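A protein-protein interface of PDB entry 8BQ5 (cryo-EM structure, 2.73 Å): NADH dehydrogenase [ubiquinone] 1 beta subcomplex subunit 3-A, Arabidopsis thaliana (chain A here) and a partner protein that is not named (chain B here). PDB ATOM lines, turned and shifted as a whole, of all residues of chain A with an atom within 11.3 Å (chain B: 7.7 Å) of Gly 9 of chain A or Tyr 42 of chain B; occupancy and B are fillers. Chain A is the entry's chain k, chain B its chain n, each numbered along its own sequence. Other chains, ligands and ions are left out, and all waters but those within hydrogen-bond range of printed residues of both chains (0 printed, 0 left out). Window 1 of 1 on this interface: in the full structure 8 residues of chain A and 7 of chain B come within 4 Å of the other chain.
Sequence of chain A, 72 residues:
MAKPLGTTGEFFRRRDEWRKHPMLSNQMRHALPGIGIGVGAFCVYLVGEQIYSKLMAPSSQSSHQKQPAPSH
Of the 17 printed residues of chain B, 7 touch a printed residue of chain A.
Hydrophobic or aromatic side chains of chain B within 4 Å of the printed part of chain A: Tyr 24, Phe 41, Tyr 42 and Ala 45.
Printed residues of chain A that touch a printed residue of chain B: Pro 4, Gly 6, Thr 8, Gly 9, Phe 12, Arg 13, Asp 16 and Arg 19.
Hydrophobic or aromatic side chains of chain A that line the printed part of chain B: Pro 4 and Phe 12.
Among the printed residues, 13 pairs touch across the chains.
Among the printed residues, Asp or Glu carboxylates within 4 Å of a Lys or Arg side-chain nitrogen of the other chain: Asp 16 of chain A with Arg 38 of chain B.
The guanidinium group (NE) of Arg 19 of chain A lies within salt-bridge range of the side-chain carboxylate (OD1) of Asp 16 of chain A.
The backbone NH (N) of Gly 9 of chain A lies within hydrogen-bond range of the side-chain hydroxyl (OG) of Ser 46 of chain B, 3.3 Å away.
The side-chain carboxylate (OD2) of Asp 16 of chain A lies close to the side-chain hydroxyl (OH) of Tyr 42 of chain B (2.4 Å).
OD1 of Asp 16 of chain A is in salt-bridge range of NH2 of Arg 38 of chain B, at 3.3 Å.
NE of Arg 38 of chain B lies close to NH2 of Arg 19 of chain A, 3.3 Å away.
CB of Pro 4 of chain A touches CB of Tyr 42 of chain B, at 3.9 Å.
Ser 46 of chain B touches Gly 6 of chain A.
Thr 8 of chain A touches Tyr 24 of chain B (OG1 to OH, 3.6 Å).
Thr 8 of chain A touches Ala 45 of chain B (CG2 to CB, 3.9 Å).
Thr 8 of chain A touches Arg 49 of chain B.
CA of Gly 9 of chain A touches O of Tyr 42 of chain B, at 3.5 Å.
Phe 12 of chain A touches Phe 41 of chain B.
C of Phe 12 of chain A touches CE1 of Tyr 42 of chain B, at 3.9 Å.
Arg 13 of chain A touches Tyr 42 of chain B.
Of the printed residues of chain B, Thr 8 of chain A touches Tyr 24 (3.6 Å), Ala 45 (3.9 Å) and Arg 49 (3.4 Å).
Of the printed residues of chain B, Asp 16 of chain A touches Arg 38 and Tyr 42.
Lys 20 of chain A touches none of the printed residues of chain B.
Of the printed residues of chain A, Tyr 24 of chain B touches Thr 8.
Arg 38 of chain B touches just these residues of chain A: Asp 16 and Arg 19.
Of chain A, only Phe 12 (3.97 Å) comes within 4 Å of Phe 41 of chain B.
Tyr 42 of chain B touches just these residues of chain A: Pro 4 (3.9 Å), Gly 9 (3.5 Å), Phe 12 (3.9 Å), Arg 13 (3.9 Å) and Asp 16 (2.4 Å).
No residue of chain A comes within 4 Å of Asp 44 of chain B.
Ala 45 of chain B touches one residue of chain A.
Ser 46 of chain B touches two residues of chain A.
Printed residues of chain A within 4 Å of Arg 49 of chain B: Thr 8 (3.4 Å).
The nearest residue of chain A that does not touch Tyr 42 of chain B is Arg 19 of chain A (5.1 Å).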
ATOM      1  N   PRO A   4      23.200 -25.521  15.284  1.00  0.00           N
ATOM      2  CA  PRO A   4      22.757 -26.338  16.428  1.00  0.00           C
ATOM      3  C   PRO A   4      23.943 -27.121  17.002  1.00  0.00           C
ATOM      4  O   PRO A   4      23.854 -28.334  17.113  1.00  0.00           O
ATOM      5  CB  PRO A   4      21.711 -27.300  15.849  1.00  0.00           C
ATOM      6  CG  PRO A   4      21.984 -27.286  14.368  1.00  0.00           C
ATOM      7  CD  PRO A   4      22.425 -25.866  14.092  1.00  0.00           C
ATOM      8  N   LEU A   5      25.016 -26.414  17.360  1.00  0.00           N
ATOM      9  CA  LEU A   5      26.200 -27.071  17.904  1.00  0.00           C
ATOM     10  C   LEU A   5      25.975 -27.508  19.348  1.00  0.00           C
ATOM     11  O   LEU A   5      26.376 -28.608  19.743  1.00  0.00           O
ATOM     12  CB  LEU A   5      27.407 -26.136  17.806  1.00  0.00           C
ATOM     13  CG  LEU A   5      28.007 -25.915  16.416  1.00  0.00           C
ATOM     14  CD1 LEU A   5      29.454 -25.456  16.526  1.00  0.00           C
ATOM     15  CD2 LEU A   5      27.902 -27.176  15.569  1.00  0.00           C
ATOM     16  N   GLY A   6      25.365 -26.653  20.168  1.00  0.00           N
ATOM     17  CA  GLY A   6      25.216 -26.970  21.605  1.00  0.00           C
ATOM     18  C   GLY A   6      24.235 -28.092  21.926  1.00  0.00           C
ATOM     19  O   GLY A   6      23.599 -28.620  20.996  1.00  0.00           O
ATOM     20  N   THR A   7      24.117 -28.445  23.214  1.00  0.00           N
ATOM     21  CA  THR A   7      23.197 -29.540  23.647  1.00  0.00           C
ATOM     22  C   THR A   7      21.756 -29.150  23.323  1.00  0.00           C
ATOM     23  O   THR A   7      21.156 -29.819  22.463  1.00  0.00           O
ATOM     24  CB  THR A   7      23.327 -29.839  25.149  1.00  0.00           C
ATOM     25  OG1 THR A   7      24.688 -30.140  25.458  1.00  0.00           O
ATOM     26  CG2 THR A   7      22.455 -30.988  25.599  1.00  0.00           C
ATOM     27  N   THR A   8      21.221 -28.124  23.996  1.00  0.00           N
ATOM     28  CA  THR A   8      19.845 -27.627  23.734  1.00  0.00           C
ATOM     29  C   THR A   8      19.618 -27.509  22.226  1.00  0.00           C
ATOM     30  O   THR A   8      18.582 -28.012  21.739  1.00  0.00           O
ATOM     31  CB  THR A   8      19.655 -26.215  24.299  1.00  0.00           C
ATOM     32  OG1 THR A   8      20.229 -26.152  25.605  1.00  0.00           O
ATOM     33  CG2 THR A   8      18.208 -25.778  24.349  1.00  0.00           C
ATOM     34  N   GLY A   9      20.544 -26.857  21.518  1.00  0.00           N
ATOM     35  CA  GLY A   9      20.361 -26.632  20.072  1.00  0.00           C
ATOM     36  C   GLY A   9      20.190 -27.922  19.294  1.00  0.00           C
ATOM     37  O   GLY A   9      19.168 -28.044  18.594  1.00  0.00           O
ATOM     38  N   GLU A  10      21.144 -28.849  19.415  1.00  0.00           N
ATOM     39  CA  GLU A  10      21.093 -30.125  18.642  1.00  0.00           C
ATOM     40  C   GLU A  10      19.873 -30.945  19.077  1.00  0.00           C
ATOM     41  O   GLU A  10      19.301 -31.630  18.221  1.00  0.00           O
ATOM     42  CB  GLU A  10      22.395 -30.912  18.813  1.00  0.00           C
ATOM     43  CG  GLU A  10      22.554 -32.091  17.865  1.00  0.00           C
ATOM     44  CD  GLU A  10      22.233 -31.855  16.396  1.00  0.00           C
ATOM     45  OE1 GLU A  10      22.824 -30.936  15.797  1.00  0.00           O
ATOM     46  OE2 GLU A  10      21.403 -32.607  15.849  1.00  0.00           O
ATOM     47  N   PHE A  11      19.489 -30.868  20.350  1.00  0.00           N
ATOM     48  CA  PHE A  11      18.273 -31.587  20.811  1.00  0.00           C
ATOM     49  C   PHE A  11      17.082 -31.173  19.951  1.00  0.00           C
ATOM     50  O   PHE A  11      16.383 -32.059  19.436  1.00  0.00           O
ATOM     51  CB  PHE A  11      17.981 -31.290  22.279  1.00  0.00           C
ATOM     52  CG  PHE A  11      16.648 -31.811  22.751  1.00  0.00           C
ATOM     53  CD1 PHE A  11      16.278 -33.127  22.520  1.00  0.00           C
ATOM     54  CD2 PHE A  11      15.761 -30.984  23.414  1.00  0.00           C
ATOM     55  CE1 PHE A  11      15.054 -33.610  22.951  1.00  0.00           C
ATOM     56  CE2 PHE A  11      14.537 -31.468  23.843  1.00  0.00           C
ATOM     57  CZ  PHE A  11      14.185 -32.777  23.609  1.00  0.00           C
ATOM     58  N   PHE A  12      16.872 -29.866  19.800  1.00  0.00           N
ATOM     59  CA  PHE A  12      15.696 -29.369  19.038  1.00  0.00           C
ATOM     60  C   PHE A  12      15.884 -29.671  17.553  1.00  0.00           C
ATOM     61  O   PHE A  12      14.875 -29.941  16.892  1.00  0.00           O
ATOM     62  CB  PHE A  12      15.446 -27.897  19.360  1.00  0.00           C
ATOM     63  CG  PHE A  12      14.807 -27.707  20.714  1.00  0.00           C
ATOM     64  CD1 PHE A  12      13.580 -28.281  21.001  1.00  0.00           C
ATOM     65  CD2 PHE A  12      15.445 -26.989  21.712  1.00  0.00           C
ATOM     66  CE1 PHE A  12      12.994 -28.123  22.247  1.00  0.00           C
ATOM     67  CE2 PHE A  12      14.858 -26.833  22.959  1.00  0.00           C
ATOM     68  CZ  PHE A  12      13.637 -27.403  23.226  1.00  0.00           C
ATOM     69  N   ARG A  13      17.127 -29.683  17.066  1.00  0.00           N
ATOM     70  CA  ARG A  13      17.364 -30.070  15.653  1.00  0.00           C
ATOM     71  C   ARG A  13      16.904 -31.517  15.457  1.00  0.00           C
ATOM     72  O   ARG A  13      16.308 -31.800  14.401  1.00  0.00           O
ATOM     73  CB  ARG A  13      18.834 -29.858  15.287  1.00  0.00           C
ATOM     74  CG  ARG A  13      19.140 -30.213  13.840  1.00  0.00           C
ATOM     75  CD  ARG A  13      20.575 -29.939  13.450  1.00  0.00           C
ATOM     76  NE  ARG A  13      20.864 -30.257  12.059  1.00  0.00           N
ATOM     77  CZ  ARG A  13      21.988 -29.929  11.436  1.00  0.00           C
ATOM     78  NH1 ARG A  13      22.932 -29.263  12.079  1.00  0.00           N
ATOM     79  NH2 ARG A  13      22.163 -30.262  10.170  1.00  0.00           N
ATOM     80  N   ARG A  14      17.153 -32.385  16.441  1.00  0.00           N
ATOM     81  CA  ARG A  14      16.691 -33.799  16.368  1.00  0.00           C
ATOM     82  C   ARG A  14      15.159 -33.864  16.391  1.00  0.00           C
ATOM     83  O   ARG A  14      14.607 -34.730  15.685  1.00  0.00           O
ATOM     84  CB  ARG A  14      17.315 -34.608  17.508  1.00  0.00           C
ATOM     85  CG  ARG A  14      18.803 -34.874  17.332  1.00  0.00           C
ATOM     86  CD  ARG A  14      19.375 -35.639  18.508  1.00  0.00           C
ATOM     87  NE  ARG A  14      20.667 -35.131  18.940  1.00  0.00           N
ATOM     88  CZ  ARG A  14      21.765 -35.868  19.069  1.00  0.00           C
ATOM     89  NH1 ARG A  14      21.738 -37.162  18.801  1.00  0.00           N
ATOM     90  NH2 ARG A  14      22.893 -35.307  19.467  1.00  0.00           N
ATOM     91  N   ARG A  15      14.502 -33.009  17.180  1.00  0.00           N
ATOM     92  CA  ARG A  15      13.047 -33.009  17.266  1.00  0.00           C
ATOM     93  C   ARG A  15      12.386 -32.540  15.977  1.00  0.00           C
ATOM     94  O   ARG A  15      11.269 -32.974  15.677  1.00  0.00           O
ATOM     95  CB  ARG A  15      12.590 -32.139  18.438  1.00  0.00           C
ATOM     96  CG  ARG A  15      13.053 -32.642  19.796  1.00  0.00           C
ATOM     97  CD  ARG A  15      12.588 -34.069  20.014  1.00  0.00           C
ATOM     98  NE  ARG A  15      11.190 -34.249  19.644  1.00  0.00           N
ATOM     99  CZ  ARG A  15      10.623 -35.425  19.416  1.00  0.00           C
ATOM    100  NH1 ARG A  15      11.321 -36.547  19.463  1.00  0.00           N
ATOM    101  NH2 ARG A  15       9.328 -35.475  19.120  1.00  0.00           N
ATOM    102  N   ASP A  16      13.049 -31.681  15.205  1.00  0.00           N
ATOM    103  CA  ASP A  16      12.480 -31.119  13.988  1.00  0.00           C
ATOM    104  C   ASP A  16      12.841 -31.918  12.739  1.00  0.00           C
ATOM    105  O   ASP A  16      12.942 -31.336  11.654  1.00  0.00           O
ATOM    106  CB  ASP A  16      12.929 -29.666  13.819  1.00  0.00           C
ATOM    107  CG  ASP A  16      12.554 -28.795  15.000  1.00  0.00           C
ATOM    108  OD1 ASP A  16      11.465 -28.997  15.576  1.00  0.00           O
ATOM    109  OD2 ASP A  16      13.348 -27.901  15.351  1.00  0.00           O
ATOM    110  N   GLU A  17      13.046 -33.232  12.866  1.00  0.00           N
ATOM    111  CA  GLU A  17      13.402 -34.028  11.696  1.00  0.00           C
ATOM    112  C   GLU A  17      12.225 -34.192  10.745  1.00  0.00           C
ATOM    113  O   GLU A  17      12.422 -34.343   9.534  1.00  0.00           O
ATOM    114  CB  GLU A  17      13.933 -35.394  12.126  1.00  0.00           C
ATOM    115  CG  GLU A  17      15.282 -35.725  11.520  1.00  0.00           C
ATOM    116  CD  GLU A  17      16.365 -34.782  11.997  1.00  0.00           C
ATOM    117  OE1 GLU A  17      16.753 -34.873  13.180  1.00  0.00           O
ATOM    118  OE2 GLU A  17      16.815 -33.937  11.195  1.00  0.00           O
ATOM    119  N   TRP A  18      10.998 -34.167  11.269  1.00  0.00           N
ATOM    120  CA  TRP A  18       9.816 -34.302  10.426  1.00  0.00           C
ATOM    121  C   TRP A  18       9.632 -33.121   9.487  1.00  0.00           C
ATOM    122  O   TRP A  18       8.918 -33.243   8.485  1.00  0.00           O
ATOM    123  CB  TRP A  18       8.575 -34.477  11.301  1.00  0.00           C
ATOM    124  CG  TRP A  18       8.229 -33.266  12.123  1.00  0.00           C
ATOM    125  CD1 TRP A  18       8.629 -33.008  13.401  1.00  0.00           C
ATOM    126  CD2 TRP A  18       7.394 -32.166  11.736  1.00  0.00           C
ATOM    127  NE1 TRP A  18       8.108 -31.813  13.829  1.00  0.00           N
ATOM    128  CE2 TRP A  18       7.345 -31.276  12.827  1.00  0.00           C
ATOM    129  CE3 TRP A  18       6.691 -31.844  10.572  1.00  0.00           C
ATOM    130  CZ2 TRP A  18       6.620 -30.089  12.790  1.00  0.00           C
ATOM    131  CZ3 TRP A  18       5.971 -30.666  10.538  1.00  0.00           C
ATOM    132  CH2 TRP A  18       5.941 -29.802  11.638  1.00  0.00           C
ATOM    133  N   ARG A  19      10.266 -31.985   9.780  1.00  0.00           N
ATOM    134  CA  ARG A  19      10.099 -30.786   8.971  1.00  0.00           C
ATOM    135  C   ARG A  19      10.737 -30.905   7.594  1.00  0.00           C
ATOM    136  O   ARG A  19      10.542 -30.013   6.763  1.00  0.00           O
ATOM    137  CB  ARG A  19      10.673 -29.580   9.711  1.00  0.00           C
ATOM    138  CG  ARG A  19       9.737 -29.011  10.766  1.00  0.00           C
ATOM    139  CD  ARG A  19      10.470 -28.086  11.714  1.00  0.00           C
ATOM    140  NE  ARG A  19       9.878 -28.076  13.045  1.00  0.00           N
ATOM    141  CZ  ARG A  19       8.881 -27.279  13.407  1.00  0.00           C
ATOM    142  NH1 ARG A  19       8.308 -26.456  12.545  1.00  0.00           N
ATOM    143  NH2 ARG A  19       8.448 -27.312  14.663  1.00  0.00           N
ATOM    144  N   LYS A  20      11.500 -31.968   7.338  1.00  0.00           N
ATOM    145  CA  LYS A  20      12.128 -32.191   6.041  1.00  0.00           C
ATOM    146  C   LYS A  20      11.205 -32.894   5.053  1.00  0.00           C
ATOM    147  O   LYS A  20      11.693 -33.498   4.088  1.00  0.00           O
ATOM    148  CB  LYS A  20      13.420 -32.993   6.215  1.00  0.00           C
ATOM    149  CG  LYS A  20      14.412 -32.374   7.191  1.00  0.00           C
ATOM    150  CD  LYS A  20      14.594 -30.885   6.932  1.00  0.00           C
ATOM    151  CE  LYS A  20      15.778 -30.324   7.704  1.00  0.00           C
ATOM    152  NZ  LYS A  20      16.643 -29.468   6.842  1.00  0.00           N
ATOM    153  N   TYR B  24      14.512 -20.112  33.340  1.00  0.00           N
ATOM    154  CA  TYR B  24      14.996 -20.763  32.129  1.00  0.00           C
ATOM    155  C   TYR B  24      13.846 -21.116  31.194  1.00  0.00           C
ATOM    156  O   TYR B  24      13.965 -20.979  29.971  1.00  0.00           O
ATOM    157  CB  TYR B  24      15.794 -22.017  32.483  1.00  0.00           C
ATOM    158  CG  TYR B  24      16.438 -22.677  31.285  1.00  0.00           C
ATOM    159  CD1 TYR B  24      17.342 -21.984  30.491  1.00  0.00           C
ATOM    160  CD2 TYR B  24      16.129 -23.984  30.938  1.00  0.00           C
ATOM    161  CE1 TYR B  24      17.928 -22.578  29.394  1.00  0.00           C
ATOM    162  CE2 TYR B  24      16.709 -24.587  29.841  1.00  0.00           C
ATOM    163  CZ  TYR B  24      17.609 -23.879  29.073  1.00  0.00           C
ATOM    164  OH  TYR B  24      18.191 -24.473  27.980  1.00  0.00           O
ATOM    165  N   THR B  31      12.850 -16.726  23.599  1.00  0.00           N
ATOM    166  CA  THR B  31      13.849 -16.800  22.538  1.00  0.00           C
ATOM    167  C   THR B  31      13.208 -17.158  21.204  1.00  0.00           C
ATOM    168  O   THR B  31      13.548 -16.578  20.166  1.00  0.00           O
ATOM    169  CB  THR B  31      14.930 -17.816  22.906  1.00  0.00           C
ATOM    170  OG1 THR B  31      15.758 -17.279  23.943  1.00  0.00           O
ATOM    171  CG2 THR B  31      15.796 -18.146  21.698  1.00  0.00           C
ATOM    172  N   LEU B  32      12.271 -18.106  21.211  1.00  0.00           N
ATOM    173  CA  LEU B  32      11.647 -18.529  19.964  1.00  0.00           C
ATOM    174  C   LEU B  32      10.694 -17.461  19.434  1.00  0.00           C
ATOM    175  O   LEU B  32      10.443 -17.390  18.226  1.00  0.00           O
ATOM    176  CB  LEU B  32      10.928 -19.863  20.172  1.00  0.00           C
ATOM    177  CG  LEU B  32      10.257 -20.512  18.962  1.00  0.00           C
ATOM    178  CD1 LEU B  32      11.246 -20.656  17.820  1.00  0.00           C
ATOM    179  CD2 LEU B  32       9.701 -21.867  19.347  1.00  0.00           C
ATOM    180  N   ALA B  35      13.067 -15.236  17.411  1.00  0.00           N
ATOM    181  CA  ALA B  35      13.746 -15.897  16.302  1.00  0.00           C
ATOM    182  C   ALA B  35      12.794 -16.457  15.256  1.00  0.00           C
ATOM    183  O   ALA B  35      13.159 -16.534  14.079  1.00  0.00           O
ATOM    184  CB  ALA B  35      14.638 -17.023  16.830  1.00  0.00           C
ATOM    185  N   HIS B  37      11.950 -18.525  13.170  1.00  0.00           N
ATOM    186  CA  HIS B  37      12.399 -19.676  12.398  1.00  0.00           C
ATOM    187  C   HIS B  37      13.082 -20.698  13.295  1.00  0.00           C
ATOM    188  O   HIS B  37      13.737 -20.343  14.280  1.00  0.00           O
ATOM    189  CB  HIS B  37      13.356 -19.234  11.293  1.00  0.00           C
ATOM    190  CG  HIS B  37      12.755 -18.256  10.336  1.00  0.00           C
ATOM    191  ND1 HIS B  37      11.422 -18.278   9.989  1.00  0.00           N
ATOM    192  CD2 HIS B  37      13.302 -17.218   9.662  1.00  0.00           C
ATOM    193  CE1 HIS B  37      11.175 -17.297   9.139  1.00  0.00           C
ATOM    194  NE2 HIS B  37      12.298 -16.639   8.926  1.00  0.00           N
ATOM    195  N   ARG B  38      12.925 -21.975  12.944  1.00  0.00           N
ATOM    196  CA  ARG B  38      13.502 -23.046  13.748  1.00  0.00           C
ATOM    197  C   ARG B  38      15.023 -22.959  13.783  1.00  0.00           C
ATOM    198  O   ARG B  38      15.639 -23.049  14.850  1.00  0.00           O
ATOM    199  CB  ARG B  38      13.063 -24.405  13.200  1.00  0.00           C
ATOM    200  CG  ARG B  38      11.566 -24.555  13.043  1.00  0.00           C
ATOM    201  CD  ARG B  38      10.861 -24.261  14.349  1.00  0.00           C
ATOM    202  NE  ARG B  38      11.052 -25.332  15.318  1.00  0.00           N
ATOM    203  CZ  ARG B  38      10.588 -25.306  16.559  1.00  0.00           C
ATOM    204  NH1 ARG B  38       9.907 -24.270  17.019  1.00  0.00           N
ATOM    205  NH2 ARG B  38      10.815 -26.344  17.358  1.00  0.00           N
ATOM    206  N   HIS B  39      15.645 -22.769  12.617  1.00  0.00           N
ATOM    207  CA  HIS B  39      17.098 -22.856  12.538  1.00  0.00           C
ATOM    208  C   HIS B  39      17.780 -21.710  13.273  1.00  0.00           C
ATOM    209  O   HIS B  39      18.827 -21.919  13.896  1.00  0.00           O
ATOM    210  CB  HIS B  39      17.540 -22.930  11.074  1.00  0.00           C
ATOM    211  CG  HIS B  39      17.493 -21.622  10.345  1.00  0.00           C
ATOM    212  ND1 HIS B  39      18.424 -20.624  10.538  1.00  0.00           N
ATOM    213  CD2 HIS B  39      16.630 -21.156   9.412  1.00  0.00           C
ATOM    214  CE1 HIS B  39      18.137 -19.602   9.752  1.00  0.00           C
ATOM    215  NE2 HIS B  39      17.049 -19.896   9.065  1.00  0.00           N
ATOM    216  N   ILE B  40      17.217 -20.502  13.219  1.00  0.00           N
ATOM    217  CA  ILE B  40      17.770 -19.422  14.026  1.00  0.00           C
ATOM    218  C   ILE B  40      17.630 -19.760  15.502  1.00  0.00           C
ATOM    219  O   ILE B  40      18.544 -19.523  16.297  1.00  0.00           O
ATOM    220  CB  ILE B  40      17.098 -18.077  13.693  1.00  0.00           C
ATOM    221  CG1 ILE B  40      17.075 -17.834  12.190  1.00  0.00           C
ATOM    222  CG2 ILE B  40      17.874 -16.947  14.320  1.00  0.00           C
ATOM    223  CD1 ILE B  40      16.243 -16.643  11.779  1.00  0.00           C
ATOM    224  N   PHE B  41      16.501 -20.369  15.875  1.00  0.00           N
ATOM    225  CA  PHE B  41      16.217 -20.649  17.278  1.00  0.00           C
ATOM    226  C   PHE B  41      17.248 -21.591  17.886  1.00  0.00           C
ATOM    227  O   PHE B  41      17.579 -21.471  19.071  1.00  0.00           O
ATOM    228  CB  PHE B  41      14.812 -21.237  17.410  1.00  0.00           C
ATOM    229  CG  PHE B  41      14.508 -21.789  18.773  1.00  0.00           C
ATOM    230  CD1 PHE B  41      14.500 -20.959  19.881  1.00  0.00           C
ATOM    231  CD2 PHE B  41      14.226 -23.133  18.947  1.00  0.00           C
ATOM    232  CE1 PHE B  41      14.220 -21.460  21.139  1.00  0.00           C
ATOM    233  CE2 PHE B  41      13.945 -23.639  20.203  1.00  0.00           C
ATOM    234  CZ  PHE B  41      13.943 -22.801  21.298  1.00  0.00           C
ATOM    235  N   TYR B  42      17.765 -22.534  17.094  1.00  0.00           N
ATOM    236  CA  TYR B  42      18.700 -23.523  17.621  1.00  0.00           C
ATOM    237  C   TYR B  42      19.921 -22.852  18.238  1.00  0.00           C
ATOM    238  O   TYR B  42      20.313 -23.158  19.369  1.00  0.00           O
ATOM    239  CB  TYR B  42      19.140 -24.486  16.518  1.00  0.00           C
ATOM    240  CG  TYR B  42      18.029 -25.219  15.809  1.00  0.00           C
ATOM    241  CD1 TYR B  42      16.852 -25.560  16.462  1.00  0.00           C
ATOM    242  CD2 TYR B  42      18.169 -25.586  14.481  1.00  0.00           C
ATOM    243  CE1 TYR B  42      15.844 -26.234  15.799  1.00  0.00           C
ATOM    244  CE2 TYR B  42      17.174 -26.255  13.814  1.00  0.00           C
ATOM    245  CZ  TYR B  42      16.014 -26.580  14.473  1.00  0.00           C
ATOM    246  OH  TYR B  42      15.027 -27.253  13.792  1.00  0.00           O
ATOM    247  N   ARG B  43      20.542 -21.930  17.500  1.00  0.00           N
ATOM    248  CA  ARG B  43      21.724 -21.266  18.032  1.00  0.00           C
ATOM    249  C   ARG B  43      21.365 -20.359  19.198  1.00  0.00           C
ATOM    250  O   ARG B  43      21.986 -20.437  20.261  1.00  0.00           O
ATOM    251  CB  ARG B  43      22.451 -20.491  16.933  1.00  0.00           C
ATOM    252  CG  ARG B  43      22.307 -21.095  15.547  1.00  0.00           C
ATOM    253  CD  ARG B  43      23.305 -20.480  14.565  1.00  0.00           C
ATOM    254  NE  ARG B  43      23.156 -19.038  14.398  1.00  0.00           N
ATOM    255  CZ  ARG B  43      22.052 -18.425  13.989  1.00  0.00           C
ATOM    256  NH1 ARG B  43      20.971 -19.102  13.641  1.00  0.00           N
ATOM    257  NH2 ARG B  43      22.039 -17.098  13.911  1.00  0.00           N
ATOM    258  N   ASP B  44      20.333 -19.526  19.042  1.00  0.00           N
ATOM    259  CA  ASP B  44      19.952 -18.631  20.130  1.00  0.00           C
ATOM    260  C   ASP B  44      19.566 -19.414  21.382  1.00  0.00           C
ATOM    261  O   ASP B  44      19.697 -18.910  22.503  1.00  0.00           O
ATOM    262  CB  ASP B  44      18.816 -17.710  19.685  1.00  0.00           C
ATOM    263  CG  ASP B  44      18.942 -17.290  18.231  1.00  0.00           C
ATOM    264  OD1 ASP B  44      17.932 -17.356  17.500  1.00  0.00           O
ATOM    265  OD2 ASP B  44      20.057 -16.914  17.816  1.00  0.00           O
ATOM    266  N   ALA B  45      19.107 -20.656  21.209  1.00  0.00           N
ATOM    267  CA  ALA B  45      18.831 -21.516  22.356  1.00  0.00           C
ATOM    268  C   ALA B  45      20.113 -21.919  23.072  1.00  0.00           C
ATOM    269  O   ALA B  45      20.143 -22.010  24.305  1.00  0.00           O
ATOM    270  CB  ALA B  45      18.062 -22.757  21.909  1.00  0.00           C
ATOM    271  N   SER B  46      21.182 -22.186  22.316  1.00  0.00           N
ATOM    272  CA  SER B  46      22.425 -22.640  22.933  1.00  0.00           C
ATOM    273  C   SER B  46      23.107 -21.517  23.702  1.00  0.00           C
ATOM    274  O   SER B  46      23.628 -21.738  24.801  1.00  0.00           O
ATOM    275  CB  SER B  46      23.358 -23.213  21.868  1.00  0.00           C
ATOM    276  OG  SER B  46      22.892 -24.475  21.421  1.00  0.00           O
ATOM    277  N   ASP B  47      23.111 -20.304  23.146  1.00  0.00           N
ATOM    278  CA  ASP B  47      23.734 -19.177  23.832  1.00  0.00           C
ATOM    279  C   ASP B  47      23.038 -18.873  25.152  1.00  0.00           C
ATOM    280  O   ASP B  47      23.694 -18.511  26.135  1.00  0.00           O
ATOM    281  CB  ASP B  47      23.738 -17.948  22.924  1.00  0.00           C
ATOM    282  CG  ASP B  47      24.711 -18.084  21.772  1.00  0.00           C
ATOM    283  OD1 ASP B  47      25.581 -18.977  21.816  1.00  0.00           O
ATOM    284  OD2 ASP B  47      24.574 -17.326  20.798  1.00  0.00           O
ATOM    285  N   LEU B  48      21.710 -19.013  25.193  1.00  0.00           N
ATOM    286  CA  LEU B  48      20.978 -18.755  26.429  1.00  0.00           C
ATOM    287  C   LEU B  48      21.267 -19.833  27.471  1.00  0.00           C
ATOM    288  O   LEU B  48      21.486 -19.525  28.649  1.00  0.00           O
ATOM    289  CB  LEU B  48      19.476 -18.647  26.137  1.00  0.00           C
ATOM    290  CG  LEU B  48      18.440 -19.013  27.204  1.00  0.00           C
ATOM    291  CD1 LEU B  48      18.429 -17.943  28.245  1.00  0.00           C
ATOM    292  CD2 LEU B  48      17.059 -19.062  26.638  1.00  0.00           C
ATOM    293  N   ARG B  49      21.285 -21.104  27.057  1.00  0.00           N
ATOM    294  CA  ARG B  49      21.691 -22.172  27.968  1.00  0.00           C
ATOM    295  C   ARG B  49      23.144 -22.002  28.390  1.00  0.00           C
ATOM    296  O   ARG B  49      23.518 -22.347  29.518  1.00  0.00           O
ATOM    297  CB  ARG B  49      21.480 -23.534  27.306  1.00  0.00           C
ATOM    298  CG  ARG B  49      21.959 -24.727  28.123  1.00  0.00           C
ATOM    299  CD  ARG B  49      21.112 -24.954  29.358  1.00  0.00           C
ATOM    300  NE  ARG B  49      21.695 -25.973  30.222  1.00  0.00           N
ATOM    301  CZ  ARG B  49      21.231 -27.210  30.327  1.00  0.00           C
ATOM    302  NH1 ARG B  49      20.195 -27.621  29.613  1.00  0.00           N
ATOM    303  NH2 ARG B  49      21.820 -28.056  31.167  1.00  0.00           N
